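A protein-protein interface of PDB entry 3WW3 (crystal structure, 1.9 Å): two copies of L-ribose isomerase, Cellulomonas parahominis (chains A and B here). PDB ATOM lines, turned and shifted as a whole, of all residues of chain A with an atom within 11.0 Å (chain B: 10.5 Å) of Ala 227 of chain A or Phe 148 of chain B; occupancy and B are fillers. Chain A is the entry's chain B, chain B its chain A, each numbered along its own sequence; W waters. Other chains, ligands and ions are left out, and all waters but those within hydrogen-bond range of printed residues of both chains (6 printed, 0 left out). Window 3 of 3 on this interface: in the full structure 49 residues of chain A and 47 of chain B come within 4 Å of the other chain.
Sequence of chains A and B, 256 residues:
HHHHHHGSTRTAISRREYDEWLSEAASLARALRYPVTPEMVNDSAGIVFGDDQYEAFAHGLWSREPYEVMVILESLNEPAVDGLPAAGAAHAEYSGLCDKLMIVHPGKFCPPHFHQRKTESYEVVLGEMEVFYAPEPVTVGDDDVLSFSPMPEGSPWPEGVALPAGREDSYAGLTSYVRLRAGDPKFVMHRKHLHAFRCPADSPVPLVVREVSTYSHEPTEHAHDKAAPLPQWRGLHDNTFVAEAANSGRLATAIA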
ATOM      1  N   LEU A  76      -8.078  -3.608  -7.633  1.00  0.00           N
ATOM      2  CA  LEU A  76      -8.583  -3.541  -6.268  1.00  0.00           C
ATOM      3  C   LEU A  76      -8.394  -2.194  -5.583  1.00  0.00           C
ATOM      4  O   LEU A  76      -7.355  -1.552  -5.722  1.00  0.00           O
ATOM      5  CB  LEU A  76      -7.881  -4.602  -5.410  1.00  0.00           C
ATOM      6  CG  LEU A  76      -8.347  -4.711  -3.956  1.00  0.00           C
ATOM      7  CD1 LEU A  76      -9.693  -5.417  -3.913  1.00  0.00           C
ATOM      8  CD2 LEU A  76      -7.318  -5.476  -3.143  1.00  0.00           C
ATOM      9  N   ASN A  77      -9.422  -1.770  -4.857  1.00  0.00           N
ATOM     10  CA  ASN A  77      -9.359  -0.555  -4.056  1.00  0.00           C
ATOM     11  C   ASN A  77     -10.417  -0.776  -2.988  1.00  0.00           C
ATOM     12  O   ASN A  77     -11.541  -0.272  -3.066  1.00  0.00           O
ATOM     13  CB  ASN A  77      -9.640   0.707  -4.872  1.00  0.00           C
ATOM     14  CG  ASN A  77      -9.148   1.960  -4.168  1.00  0.00           C
ATOM     15  OD1 ASN A  77      -8.122   1.932  -3.482  1.00  0.00           O
ATOM     16  ND2 ASN A  77      -9.864   3.066  -4.339  1.00  0.00           N
ATOM     17  N   GLU A  78     -10.019  -1.577  -2.005  1.00  0.00           N
ATOM     18  CA  GLU A  78     -10.847  -1.994  -0.881  1.00  0.00           C
ATOM     19  C   GLU A  78     -10.606  -1.157   0.372  1.00  0.00           C
ATOM     20  O   GLU A  78      -9.488  -1.095   0.881  1.00  0.00           O
ATOM     21  CB  GLU A  78     -10.548  -3.471  -0.598  1.00  0.00           C
ATOM     22  CG  GLU A  78     -11.091  -4.013   0.709  1.00  0.00           C
ATOM     23  CD  GLU A  78     -12.591  -3.899   0.806  1.00  0.00           C
ATOM     24  OE1 GLU A  78     -13.277  -4.273  -0.163  1.00  0.00           O
ATOM     25  OE2 GLU A  78     -13.083  -3.442   1.857  1.00  0.00           O
ATOM     26  N   PRO A  79     -11.662  -0.507   0.889  1.00  0.00           N
ATOM     27  CA  PRO A  79     -11.571   0.332   2.087  1.00  0.00           C
ATOM     28  C   PRO A  79     -11.104  -0.427   3.327  1.00  0.00           C
ATOM     29  O   PRO A  79     -10.412   0.128   4.178  1.00  0.00           O
ATOM     30  CB  PRO A  79     -12.996   0.857   2.247  1.00  0.00           C
ATOM     31  CG  PRO A  79     -13.506   0.892   0.847  1.00  0.00           C
ATOM     32  CD  PRO A  79     -13.006  -0.419   0.295  1.00  0.00           C
ATOM     33  N   ALA A  80     -11.481  -1.699   3.419  1.00  0.00           N
ATOM     34  CA  ALA A  80     -11.127  -2.531   4.568  1.00  0.00           C
ATOM     35  C   ALA A  80     -11.661  -1.885   5.836  1.00  0.00           C
ATOM     36  O   ALA A  80     -11.024  -1.924   6.892  1.00  0.00           O
ATOM     37  CB  ALA A  80      -9.612  -2.707   4.663  1.00  0.00           C
ATOM     38  N   VAL A  81     -12.835  -1.277   5.724  1.00  0.00           N
ATOM     39  CA  VAL A  81     -13.468  -0.639   6.868  1.00  0.00           C
ATOM     40  C   VAL A  81     -14.322  -1.665   7.615  1.00  0.00           C
ATOM     41  O   VAL A  81     -14.498  -1.569   8.829  1.00  0.00           O
ATOM     42  CB  VAL A  81     -14.335   0.550   6.417  1.00  0.00           C
ATOM     43  CG1 VAL A  81     -15.240   1.004   7.539  1.00  0.00           C
ATOM     44  CG2 VAL A  81     -13.428   1.703   5.995  1.00  0.00           C
ATOM     45  N   ASP A  82     -14.837  -2.653   6.889  1.00  0.00           N
ATOM     46  CA  ASP A  82     -15.661  -3.688   7.508  1.00  0.00           C
ATOM     47  C   ASP A  82     -14.892  -4.424   8.602  1.00  0.00           C
ATOM     48  O   ASP A  82     -13.758  -4.862   8.392  1.00  0.00           O
ATOM     49  CB  ASP A  82     -16.151  -4.691   6.458  1.00  0.00           C
ATOM     50  CG  ASP A  82     -17.262  -4.130   5.587  1.00  0.00           C
ATOM     51  OD1 ASP A  82     -16.964  -3.455   4.577  1.00  0.00           O
ATOM     52  OD2 ASP A  82     -18.445  -4.357   5.922  1.00  0.00           O
ATOM     53  N   GLY A  83     -15.512  -4.550   9.773  1.00  0.00           N
ATOM     54  CA  GLY A  83     -14.870  -5.238  10.884  1.00  0.00           C
ATOM     55  C   GLY A  83     -13.938  -4.362  11.703  1.00  0.00           C
ATOM     56  O   GLY A  83     -13.467  -4.766  12.767  1.00  0.00           O
ATOM     57  N   LEU A  84     -13.663  -3.160  11.211  1.00  0.00           N
ATOM     58  CA  LEU A  84     -12.774  -2.234  11.903  1.00  0.00           C
ATOM     59  C   LEU A  84     -13.503  -1.647  13.114  1.00  0.00           C
ATOM     60  O   LEU A  84     -14.655  -1.221  12.999  1.00  0.00           O
ATOM     61  CB  LEU A  84     -12.373  -1.097  10.953  1.00  0.00           C
ATOM     62  CG  LEU A  84     -10.997  -0.417  10.995  1.00  0.00           C
ATOM     63  CD1 LEU A  84     -11.198   1.097  10.968  1.00  0.00           C
ATOM     64  CD2 LEU A  84     -10.204  -0.825  12.215  1.00  0.00           C
ATOM     65  N   PRO A  85     -12.855  -1.640  14.293  1.00  0.00           N
ATOM     66  CA  PRO A  85     -13.516  -1.078  15.474  1.00  0.00           C
ATOM     67  C   PRO A  85     -13.868   0.377  15.196  1.00  0.00           C
ATOM     68  O   PRO A  85     -13.060   1.111  14.623  1.00  0.00           O
ATOM     69  CB  PRO A  85     -12.451  -1.203  16.557  1.00  0.00           C
ATOM     70  CG  PRO A  85     -11.729  -2.456  16.164  1.00  0.00           C
ATOM     71  CD  PRO A  85     -11.581  -2.283  14.665  1.00  0.00           C
ATOM     72  N   ALA A  92      -8.874   5.126   9.498  1.00  0.00           N
ATOM     73  CA  ALA A  92      -9.107   4.030   8.565  1.00  0.00           C
ATOM     74  C   ALA A  92      -8.626   4.439   7.174  1.00  0.00           C
ATOM     75  O   ALA A  92      -8.238   3.594   6.367  1.00  0.00           O
ATOM     76  CB  ALA A  92     -10.594   3.684   8.526  1.00  0.00           C
ATOM     77  N   GLY A  96      -6.641   0.215   4.270  1.00  0.00           N
ATOM     78  CA  GLY A  96      -7.275  -0.228   3.042  1.00  0.00           C
ATOM     79  C   GLY A  96      -6.281  -0.977   2.172  1.00  0.00           C
ATOM     80  O   GLY A  96      -5.104  -1.082   2.519  1.00  0.00           O
ATOM     81  N   LEU A  97      -6.748  -1.488   1.036  1.00  0.00           N
ATOM     82  CA  LEU A  97      -5.894  -2.241   0.132  1.00  0.00           C
ATOM     83  C   LEU A  97      -6.169  -1.873  -1.319  1.00  0.00           C
ATOM     84  O   LEU A  97      -7.314  -1.891  -1.773  1.00  0.00           O
ATOM     85  CB  LEU A  97      -6.123  -3.743   0.334  1.00  0.00           C
ATOM     86  CG  LEU A  97      -5.895  -4.263   1.759  1.00  0.00           C
ATOM     87  CD1 LEU A  97      -6.488  -5.657   1.909  1.00  0.00           C
ATOM     88  CD2 LEU A  97      -4.413  -4.270   2.067  1.00  0.00           C
ATOM     89  N   TYR A 215      -5.445   2.182   0.685  1.00  0.00           N
ATOM     90  CA  TYR A 215      -6.522   2.748  -0.128  1.00  0.00           C
ATOM     91  C   TYR A 215      -6.156   3.991  -0.947  1.00  0.00           C
ATOM     92  O   TYR A 215      -5.472   4.887  -0.462  1.00  0.00           O
ATOM     93  CB  TYR A 215      -7.719   3.063   0.763  1.00  0.00           C
ATOM     94  CG  TYR A 215      -8.995   3.337   0.005  1.00  0.00           C
ATOM     95  CD1 TYR A 215      -9.762   2.295  -0.523  1.00  0.00           C
ATOM     96  CD2 TYR A 215      -9.454   4.642  -0.164  1.00  0.00           C
ATOM     97  CE1 TYR A 215     -10.959   2.550  -1.196  1.00  0.00           C
ATOM     98  CE2 TYR A 215     -10.644   4.907  -0.831  1.00  0.00           C
ATOM     99  CZ  TYR A 215     -11.392   3.860  -1.342  1.00  0.00           C
ATOM    100  OH  TYR A 215     -12.574   4.135  -1.990  1.00  0.00           O
ATOM    101  N   HIS A 217      -7.410   7.266  -2.407  1.00  0.00           N
ATOM    102  CA  HIS A 217      -8.463   8.274  -2.345  1.00  0.00           C
ATOM    103  C   HIS A 217      -8.298   9.165  -3.572  1.00  0.00           C
ATOM    104  O   HIS A 217      -7.499  10.103  -3.567  1.00  0.00           O
ATOM    105  CB  HIS A 217      -8.318   9.122  -1.076  1.00  0.00           C
ATOM    106  CG  HIS A 217      -8.387   8.334   0.197  1.00  0.00           C
ATOM    107  ND1 HIS A 217      -9.580   7.955   0.776  1.00  0.00           N
ATOM    108  CD2 HIS A 217      -7.409   7.863   1.008  1.00  0.00           C
ATOM    109  CE1 HIS A 217      -9.333   7.287   1.890  1.00  0.00           C
ATOM    110  NE2 HIS A 217      -8.024   7.218   2.052  1.00  0.00           N
ATOM    111  N   THR A 220     -13.629   9.492  -8.776  1.00  0.00           N
ATOM    112  CA  THR A 220     -14.090   8.472  -9.715  1.00  0.00           C
ATOM    113  C   THR A 220     -15.599   8.257  -9.612  1.00  0.00           C
ATOM    114  O   THR A 220     -16.207   8.518  -8.572  1.00  0.00           O
ATOM    115  CB  THR A 220     -13.387   7.119  -9.469  1.00  0.00           C
ATOM    116  OG1 THR A 220     -13.870   6.154 -10.412  1.00  0.00           O
ATOM    117  CG2 THR A 220     -13.658   6.621  -8.056  1.00  0.00           C
ATOM    118  N   ALA A 227     -22.500   7.217  -0.927  1.00  0.00           N
ATOM    119  CA  ALA A 227     -22.206   5.799  -0.772  1.00  0.00           C
ATOM    120  C   ALA A 227     -20.706   5.564  -0.576  1.00  0.00           C
ATOM    121  O   ALA A 227     -20.124   4.668  -1.188  1.00  0.00           O
ATOM    122  CB  ALA A 227     -22.688   5.027  -2.002  1.00  0.00           C
ATOM    123  N   ALA A 228     -20.084   6.379   0.272  1.00  0.00           N
ATOM    124  CA  ALA A 228     -18.657   6.255   0.541  1.00  0.00           C
ATOM    125  C   ALA A 228     -18.413   5.293   1.701  1.00  0.00           C
ATOM    126  O   ALA A 228     -19.290   5.084   2.540  1.00  0.00           O
ATOM    127  CB  ALA A 228     -18.068   7.621   0.862  1.00  0.00           C
ATOM    128  N   PRO A 229     -17.212   4.695   1.764  1.00  0.00           N
ATOM    129  CA  PRO A 229     -16.862   3.752   2.832  1.00  0.00           C
ATOM    130  C   PRO A 229     -17.146   4.360   4.200  1.00  0.00           C
ATOM    131  O   PRO A 229     -17.641   3.689   5.105  1.00  0.00           O
ATOM    132  CB  PRO A 229     -15.370   3.515   2.605  1.00  0.00           C
ATOM    133  CG  PRO A 229     -15.236   3.665   1.118  1.00  0.00           C
ATOM    134  CD  PRO A 229     -16.077   4.888   0.844  1.00  0.00           C
ATOM    135  N   LEU A 230     -16.825   5.643   4.330  1.00  0.00           N
ATOM    136  CA  LEU A 230     -17.035   6.383   5.567  1.00  0.00           C
ATOM    137  C   LEU A 230     -17.369   7.816   5.176  1.00  0.00           C
ATOM    138  O   LEU A 230     -16.835   8.340   4.199  1.00  0.00           O
ATOM    139  CB  LEU A 230     -15.764   6.351   6.417  1.00  0.00           C
ATOM    140  CG  LEU A 230     -15.802   5.724   7.812  1.00  0.00           C
ATOM    141  CD1 LEU A 230     -16.609   4.437   7.807  1.00  0.00           C
ATOM    142  CD2 LEU A 230     -14.378   5.468   8.272  1.00  0.00           C
ATOM    143  N   PRO A 231     -18.267   8.468   5.928  1.00  0.00           N
ATOM    144  CA  PRO A 231     -18.655   9.849   5.631  1.00  0.00           C
ATOM    145  C   PRO A 231     -17.466  10.785   5.419  1.00  0.00           C
ATOM    146  O   PRO A 231     -17.454  11.579   4.477  1.00  0.00           O
ATOM    147  CB  PRO A 231     -19.488  10.234   6.849  1.00  0.00           C
ATOM    148  CG  PRO A 231     -20.144   8.931   7.209  1.00  0.00           C
ATOM    149  CD  PRO A 231     -18.999   7.957   7.101  1.00  0.00           C
ATOM    150  N   GLN A 232     -16.468  10.683   6.291  1.00  0.00           N
ATOM    151  CA  GLN A 232     -15.286  11.533   6.202  1.00  0.00           C
ATOM    152  C   GLN A 232     -14.474  11.295   4.925  1.00  0.00           C
ATOM    153  O   GLN A 232     -13.615  12.104   4.572  1.00  0.00           O
ATOM    154  CB  GLN A 232     -14.375  11.313   7.415  1.00  0.00           C
ATOM    155  CG  GLN A 232     -15.072  11.353   8.770  1.00  0.00           C
ATOM    156  CD  GLN A 232     -15.554   9.983   9.223  1.00  0.00           C
ATOM    157  OE1 GLN A 232     -16.451   9.393   8.620  1.00  0.00           O
ATOM    158  NE2 GLN A 232     -14.950   9.470  10.293  1.00  0.00           N
ATOM    159  N   TRP A 233     -14.744  10.191   4.236  1.00  0.00           N
ATOM    160  CA  TRP A 233     -14.014   9.860   3.014  1.00  0.00           C
ATOM    161  C   TRP A 233     -14.553  10.583   1.781  1.00  0.00           C
ATOM    162  O   TRP A 233     -13.888  10.629   0.746  1.00  0.00           O
ATOM    163  CB  TRP A 233     -14.046   8.346   2.776  1.00  0.00           C
ATOM    164  CG  TRP A 233     -13.195   7.548   3.731  1.00  0.00           C
ATOM    165  CD1 TRP A 233     -12.934   7.839   5.040  1.00  0.00           C
ATOM    166  CD2 TRP A 233     -12.543   6.300   3.462  1.00  0.00           C
ATOM    167  NE1 TRP A 233     -12.163   6.851   5.603  1.00  0.00           N
ATOM    168  CE2 TRP A 233     -11.908   5.893   4.657  1.00  0.00           C
ATOM    169  CE3 TRP A 233     -12.435   5.486   2.327  1.00  0.00           C
ATOM    170  CZ2 TRP A 233     -11.175   4.704   4.752  1.00  0.00           C
ATOM    171  CZ3 TRP A 233     -11.706   4.302   2.420  1.00  0.00           C
ATOM    172  CH2 TRP A 233     -11.086   3.925   3.626  1.00  0.00           C
ATOM    173  N   ARG A 234     -15.755  11.141   1.889  1.00  0.00           N
ATOM    174  CA  ARG A 234     -16.356  11.852   0.763  1.00  0.00           C
ATOM    175  C   ARG A 234     -15.561  13.105   0.405  1.00  0.00           C
ATOM    176  O   ARG A 234     -15.219  13.905   1.277  1.00  0.00           O
ATOM    177  CB  ARG A 234     -17.807  12.240   1.078  1.00  0.00           C
ATOM    178  CG  ARG A 234     -18.433  13.149   0.021  1.00  0.00           C
ATOM    179  CD  ARG A 234     -19.918  13.422   0.259  1.00  0.00           C
ATOM    180  NE  ARG A 234     -20.773  12.372  -0.290  1.00  0.00           N
ATOM    181  CZ  ARG A 234     -20.918  11.160   0.236  1.00  0.00           C
ATOM    182  NH1 ARG A 234     -20.265  10.830   1.342  1.00  0.00           N
ATOM    183  NH2 ARG A 234     -21.713  10.274  -0.348  1.00  0.00           N
ATOM    184  N   GLY A 235     -15.273  13.258  -0.885  1.00  0.00           N
ATOM    185  CA  GLY A 235     -14.527  14.411  -1.363  1.00  0.00           C
ATOM    186  C   GLY A 235     -13.101  14.461  -0.851  1.00  0.00           C
ATOM    187  O   GLY A 235     -12.524  15.537  -0.690  1.00  0.00           O
ATOM    188  N   PRO B 137     -19.973 -12.006  10.007  1.00  0.00           N
ATOM    189  CA  PRO B 137     -18.749 -11.869  10.798  1.00  0.00           C
ATOM    190  C   PRO B 137     -18.893 -12.269  12.257  1.00  0.00           C
ATOM    191  O   PRO B 137     -19.980 -12.204  12.829  1.00  0.00           O
ATOM    192  CB  PRO B 137     -18.420 -10.389  10.658  1.00  0.00           C
ATOM    193  CG  PRO B 137     -19.775  -9.768  10.636  1.00  0.00           C
ATOM    194  CD  PRO B 137     -20.539 -10.682   9.692  1.00  0.00           C
ATOM    195  N   VAL B 145     -18.315  -2.099  15.625  1.00  0.00           N
ATOM    196  CA  VAL B 145     -17.418  -2.142  14.483  1.00  0.00           C
ATOM    197  C   VAL B 145     -18.084  -1.457  13.300  1.00  0.00           C
ATOM    198  O   VAL B 145     -19.304  -1.269  13.285  1.00  0.00           O
ATOM    199  CB  VAL B 145     -17.070  -3.597  14.090  1.00  0.00           C
ATOM    200  CG1 VAL B 145     -16.301  -4.268  15.216  1.00  0.00           C
ATOM    201  CG2 VAL B 145     -18.342  -4.374  13.782  1.00  0.00           C
ATOM    202  N   LEU B 146     -17.279  -1.086  12.314  1.00  0.00           N
ATOM    203  CA  LEU B 146     -17.787  -0.419  11.123  1.00  0.00           C
ATOM    204  C   LEU B 146     -18.253  -1.435  10.096  1.00  0.00           C
ATOM    205  O   LEU B 146     -17.870  -2.605  10.146  1.00  0.00           O
ATOM    206  CB  LEU B 146     -16.696   0.462  10.513  1.00  0.00           C
ATOM    207  CG  LEU B 146     -16.106   1.526  11.436  1.00  0.00           C
ATOM    208  CD1 LEU B 146     -14.993   2.268  10.718  1.00  0.00           C
ATOM    209  CD2 LEU B 146     -17.206   2.489  11.869  1.00  0.00           C
ATOM    210  N   SER B 147     -19.083  -0.978   9.166  1.00  0.00           N
ATOM    211  CA  SER B 147     -19.601  -1.834   8.108  1.00  0.00           C
ATOM    212  C   SER B 147     -19.784  -1.011   6.836  1.00  0.00           C
ATOM    213  O   SER B 147     -20.173   0.154   6.894  1.00  0.00           O
ATOM    214  CB  SER B 147     -20.939  -2.444   8.533  1.00  0.00           C
ATOM    215  OG  SER B 147     -21.446  -3.302   7.528  1.00  0.00           O
ATOM    216  N   PHE B 148     -19.476  -1.608   5.689  1.00  0.00           N
ATOM    217  CA  PHE B 148     -19.622  -0.910   4.416  1.00  0.00           C
ATOM    218  C   PHE B 148     -20.050  -1.822   3.278  1.00  0.00           C
ATOM    219  O   PHE B 148     -21.096  -1.616   2.655  1.00  0.00           O
ATOM    220  CB  PHE B 148     -18.313  -0.222   4.030  1.00  0.00           C
ATOM    221  CG  PHE B 148     -18.327   0.366   2.648  1.00  0.00           C
ATOM    222  CD1 PHE B 148     -19.270   1.329   2.302  1.00  0.00           C
ATOM    223  CD2 PHE B 148     -17.414  -0.055   1.689  1.00  0.00           C
ATOM    224  CE1 PHE B 148     -19.301   1.870   1.019  1.00  0.00           C
ATOM    225  CE2 PHE B 148     -17.436   0.480   0.400  1.00  0.00           C
ATOM    226  CZ  PHE B 148     -18.382   1.443   0.064  1.00  0.00           C
ATOM    227  N   SER B 149     -19.225  -2.826   3.004  1.00  0.00           N
ATOM    228  CA  SER B 149     -19.491  -3.773   1.929  1.00  0.00           C
ATOM    229  C   SER B 149     -19.468  -5.203   2.465  1.00  0.00           C
ATOM    230  O   SER B 149     -18.483  -5.921   2.302  1.00  0.00           O
ATOM    231  CB  SER B 149     -18.436  -3.604   0.830  1.00  0.00           C
ATOM    232  OG  SER B 149     -18.706  -4.443  -0.281  1.00  0.00           O
ATOM    233  N   PRO B 150     -20.565  -5.635   3.111  1.00  0.00           N
ATOM    234  CA  PRO B 150     -20.697  -6.977   3.686  1.00  0.00           C
ATOM    235  C   PRO B 150     -20.299  -8.085   2.717  1.00  0.00           C
ATOM    236  O   PRO B 150     -20.401  -7.922   1.502  1.00  0.00           O
ATOM    237  CB  PRO B 150     -22.176  -7.046   4.055  1.00  0.00           C
ATOM    238  CG  PRO B 150     -22.493  -5.637   4.404  1.00  0.00           C
ATOM    239  CD  PRO B 150     -21.806  -4.864   3.301  1.00  0.00           C
ATOM    240  N   MET B 151     -19.838  -9.210   3.258  1.00  0.00           N
ATOM    241  CA  MET B 151     -19.452 -10.340   2.421  1.00  0.00           C
ATOM    242  C   MET B 151     -20.680 -10.819   1.664  1.00  0.00           C
ATOM    243  O   MET B 151     -21.775 -10.871   2.226  1.00  0.00           O
ATOM    244  CB  MET B 151     -18.916 -11.495   3.275  1.00  0.00           C
ATOM    245  CG  MET B 151     -17.561 -11.244   3.914  1.00  0.00           C
ATOM    246  SD  MET B 151     -16.267 -10.986   2.685  1.00  0.00           S
ATOM    247  CE  MET B 151     -16.066 -12.669   2.040  1.00  0.00           C
ATOM    248  N   PRO B 152     -20.517 -11.163   0.376  1.00  0.00           N
ATOM    249  CA  PRO B 152     -21.646 -11.642  -0.427  1.00  0.00           C
ATOM    250  C   PRO B 152     -22.022 -13.045   0.041  1.00  0.00           C
ATOM    251  O   PRO B 152     -21.231 -13.708   0.710  1.00  0.00           O
ATOM    252  CB  PRO B 152     -21.088 -11.633  -1.846  1.00  0.00           C
ATOM    253  CG  PRO B 152     -19.651 -11.986  -1.631  1.00  0.00           C
ATOM    254  CD  PRO B 152     -19.277 -11.141  -0.421  1.00  0.00           C
ATOM    255  N   VAL B 188     -12.564 -10.336  -2.012  1.00  0.00           N
ATOM    256  CA  VAL B 188     -12.206  -9.855  -0.680  1.00  0.00           C
ATOM    257  C   VAL B 188     -12.793 -10.671   0.469  1.00  0.00           C
ATOM    258  O   VAL B 188     -13.983 -10.983   0.471  1.00  0.00           O
ATOM    259  CB  VAL B 188     -12.654  -8.387  -0.495  1.00  0.00           C
ATOM    260  CG1 VAL B 188     -12.464  -7.956   0.948  1.00  0.00           C
ATOM    261  CG2 VAL B 188     -11.855  -7.479  -1.419  1.00  0.00           C
ATOM    262  N   HIS B 190     -13.167 -10.133   4.253  1.00  0.00           N
ATOM    263  CA  HIS B 190     -13.060  -9.207   5.372  1.00  0.00           C
ATOM    264  C   HIS B 190     -12.606  -9.894   6.654  1.00  0.00           C
ATOM    265  O   HIS B 190     -12.888 -11.073   6.880  1.00  0.00           O
ATOM    266  CB  HIS B 190     -14.404  -8.519   5.637  1.00  0.00           C
ATOM    267  CG  HIS B 190     -14.810  -7.539   4.580  1.00  0.00           C
ATOM    268  ND1 HIS B 190     -13.966  -6.554   4.114  1.00  0.00           N
ATOM    269  CD2 HIS B 190     -15.978  -7.379   3.915  1.00  0.00           C
ATOM    270  CE1 HIS B 190     -14.596  -5.829   3.206  1.00  0.00           C
ATOM    271  NE2 HIS B 190     -15.820  -6.308   3.067  1.00  0.00           N
ATOM    272  N   ARG B 191     -11.903  -9.137   7.489  1.00  0.00           N
ATOM    273  CA  ARG B 191     -11.430  -9.631   8.773  1.00  0.00           C
ATOM    274  C   ARG B 191     -12.645 -10.126   9.564  1.00  0.00           C
ATOM    275  O   ARG B 191     -13.775  -9.731   9.286  1.00  0.00           O
ATOM    276  CB  ARG B 191     -10.744  -8.495   9.540  1.00  0.00           C
ATOM    277  CG  ARG B 191     -11.625  -7.252   9.705  1.00  0.00           C
ATOM    278  CD  ARG B 191     -10.972  -6.204  10.587  1.00  0.00           C
ATOM    279  NE  ARG B 191      -9.820  -5.559   9.954  1.00  0.00           N
ATOM    280  CZ  ARG B 191      -9.897  -4.505   9.148  1.00  0.00           C
ATOM    281  NH1 ARG B 191     -11.077  -3.965   8.865  1.00  0.00           N
ATOM    282  NH2 ARG B 191      -8.789  -3.971   8.644  1.00  0.00           N
ATOM    283  N   HIS B 193     -14.012 -13.042   9.557  1.00  0.00           N
ATOM    284  CA  HIS B 193     -14.866 -13.941   8.799  1.00  0.00           C
ATOM    285  C   HIS B 193     -14.197 -15.296   8.725  1.00  0.00           C
ATOM    286  O   HIS B 193     -13.023 -15.398   8.360  1.00  0.00           O
ATOM    287  CB  HIS B 193     -15.102 -13.405   7.386  1.00  0.00           C
ATOM    288  CG  HIS B 193     -16.165 -12.356   7.313  1.00  0.00           C
ATOM    289  ND1 HIS B 193     -17.493 -12.656   7.097  1.00  0.00           N
ATOM    290  CD2 HIS B 193     -16.103 -11.013   7.474  1.00  0.00           C
ATOM    291  CE1 HIS B 193     -18.204 -11.542   7.130  1.00  0.00           C
ATOM    292  NE2 HIS B 193     -17.384 -10.533   7.358  1.00  0.00           N
HETATM  293  O   HOH W   1      -8.207  -1.099   8.253  1.00  0.00           O
HETATM  294  O   HOH W   2     -19.526  -6.216   7.372  1.00  0.00           O
HETATM  295  O   HOH W   3     -15.488  -5.536  -0.362  1.00  0.00           O
HETATM  296  O   HOH W   4     -16.134  -7.643   8.954  1.00  0.00           O
HETATM  297  O   HOH W   5     -20.152   2.671   5.869  1.00  0.00           O
HETATM  298  O   HOH W   6     -12.312  -5.267   6.012  1.00  0.00           O
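NE2 of His 190 of chain B is in hydrogen-bond range of OD1 of Asp 82 of chain A, 3.4 Å away.
The guanidinium group (NH1) of Arg 191 of chain B sits at hydrogen-bond distance from the backbone carbonyl oxygen (O) of Asp 82 of chain A (2.9 Å).
The backbone carbonyl oxygen (O) of Leu 84 of chain A is in hydrogen-bond range of the backbone NH (N) of Leu 146 of chain B (2.7 Å).
The backbone NH (N) of Gly 83 of chain A lies within hydrogen-bond range of the backbone carbonyl oxygen (O) of Leu 146 of chain B.
The backbone NH (N) of Ser 149 of chain B is in hydrogen-bond range of the side-chain carboxylate (OD1) of Asp 82 of chain A, at 2.8 Å.
O of Ala 80 of chain A lies within hydrogen-bond range of NH1 of Arg 191 of chain B, at 2.8 Å.
N of Phe 148 of chain B is in hydrogen-bond range of OD2 of Asp 82 of chain A, at 2.9 Å.
The side-chain sulfur of Met 151 of chain B is in hydrogen-bond range of the backbone NH of His 190 of chain B (3.6 Å).
OE2 of Glu 78 of chain A sits at hydrogen-bond distance from N of Ala 80 of chain A.
O of Ser 149 of chain B is in hydrogen-bond range of NE2 of His 190 of chain B, at 2.8 Å.
N of Glu 78 of chain A lies within hydrogen-bond range of O of Leu 97 of chain A, at 2.7 Å.
OE1 of Glu 78 of chain A touches CG2 of Val 188 of chain B, 3.7 Å away.
CG1 of Val 81 of chain A touches CB of Leu 146 of chain B, 3.4 Å away.
Ser 147 of chain B touches Asp 82 of chain A (CA to OD2, 3.5 Å).
CG1 of Val 145 of chain B touches O of Gly 83 of chain A, at 3.8 Å.
Pro 229 of chain A touches Phe 148 of chain B (CA to CD1, 3.5 Å).
Phe 148 of chain B touches five residues of chain A.
Val 81 of chain A touches one residue of chain B.
Of chain A, only Asp 82 (3.5 Å) comes within 4 Å of Ser 147 of chain B.
Of the printed residues of chain A, Ser 149 of chain B touches Asp 82 (2.8 Å).
Pro 150 of chain B touches just one residue of chain A: Asp 82 (3.7 Å).
Printed residues of chain B within 4 Å of Leu 230 of chain A: Leu 146.
Of the printed residues of chain A, Val 145 of chain B touches Gly 83 (3.8 Å) and Leu 84 (3.3 Å).
Of the printed residues of chain A, Leu 146 of chain B touches Val 81 (3.4 Å), Asp 82 (3.6 Å), Gly 83 (3.1 Å), Leu 84 (2.7 Å) and Leu 230 (3.97 Å).
The nearest residue of chain B that does not touch Ala 227 of chain A is Ser 149 of chain B (8.6 Å).
The nearest printed residue of chain A that does not touch Arg 191 of chain B is Val 81 of chain A (4.2 Å).
Hydrophobic or aromatic side chains of chain B within 4 Å of the printed part of chain A: Val 145, Leu 146, Phe 148, Val 188 and His 190.
Hydrophobic or aromatic side chains of chain A within 4 Å of the printed part of chain B: Leu 76, Pro 79, Val 81, Leu 84, Pro 229 and Leu 230.
Among the printed residues, no Asp or Glu carboxylate lies within 4 Å of a Lys or Arg side-chain nitrogen of the other chain.
No position is printed for both chains.
Of the 23 pairs that touch across the chains among the printed residues, none has its exchanged pair printed and touching as well.
Water W5 bridges the backbone carbonyl oxygen (O) of Ser 147 of chain B and the backbone carbonyl oxygen (O) of Pro 229 of chain A.
Water W6 lies within hydrogen-bond range of the backbone carbonyl oxygen of Asp 82 of chain A, a ring nitrogen (ND1) of His 190 of chain B and the guanidinium group of Arg 191 of chain B.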
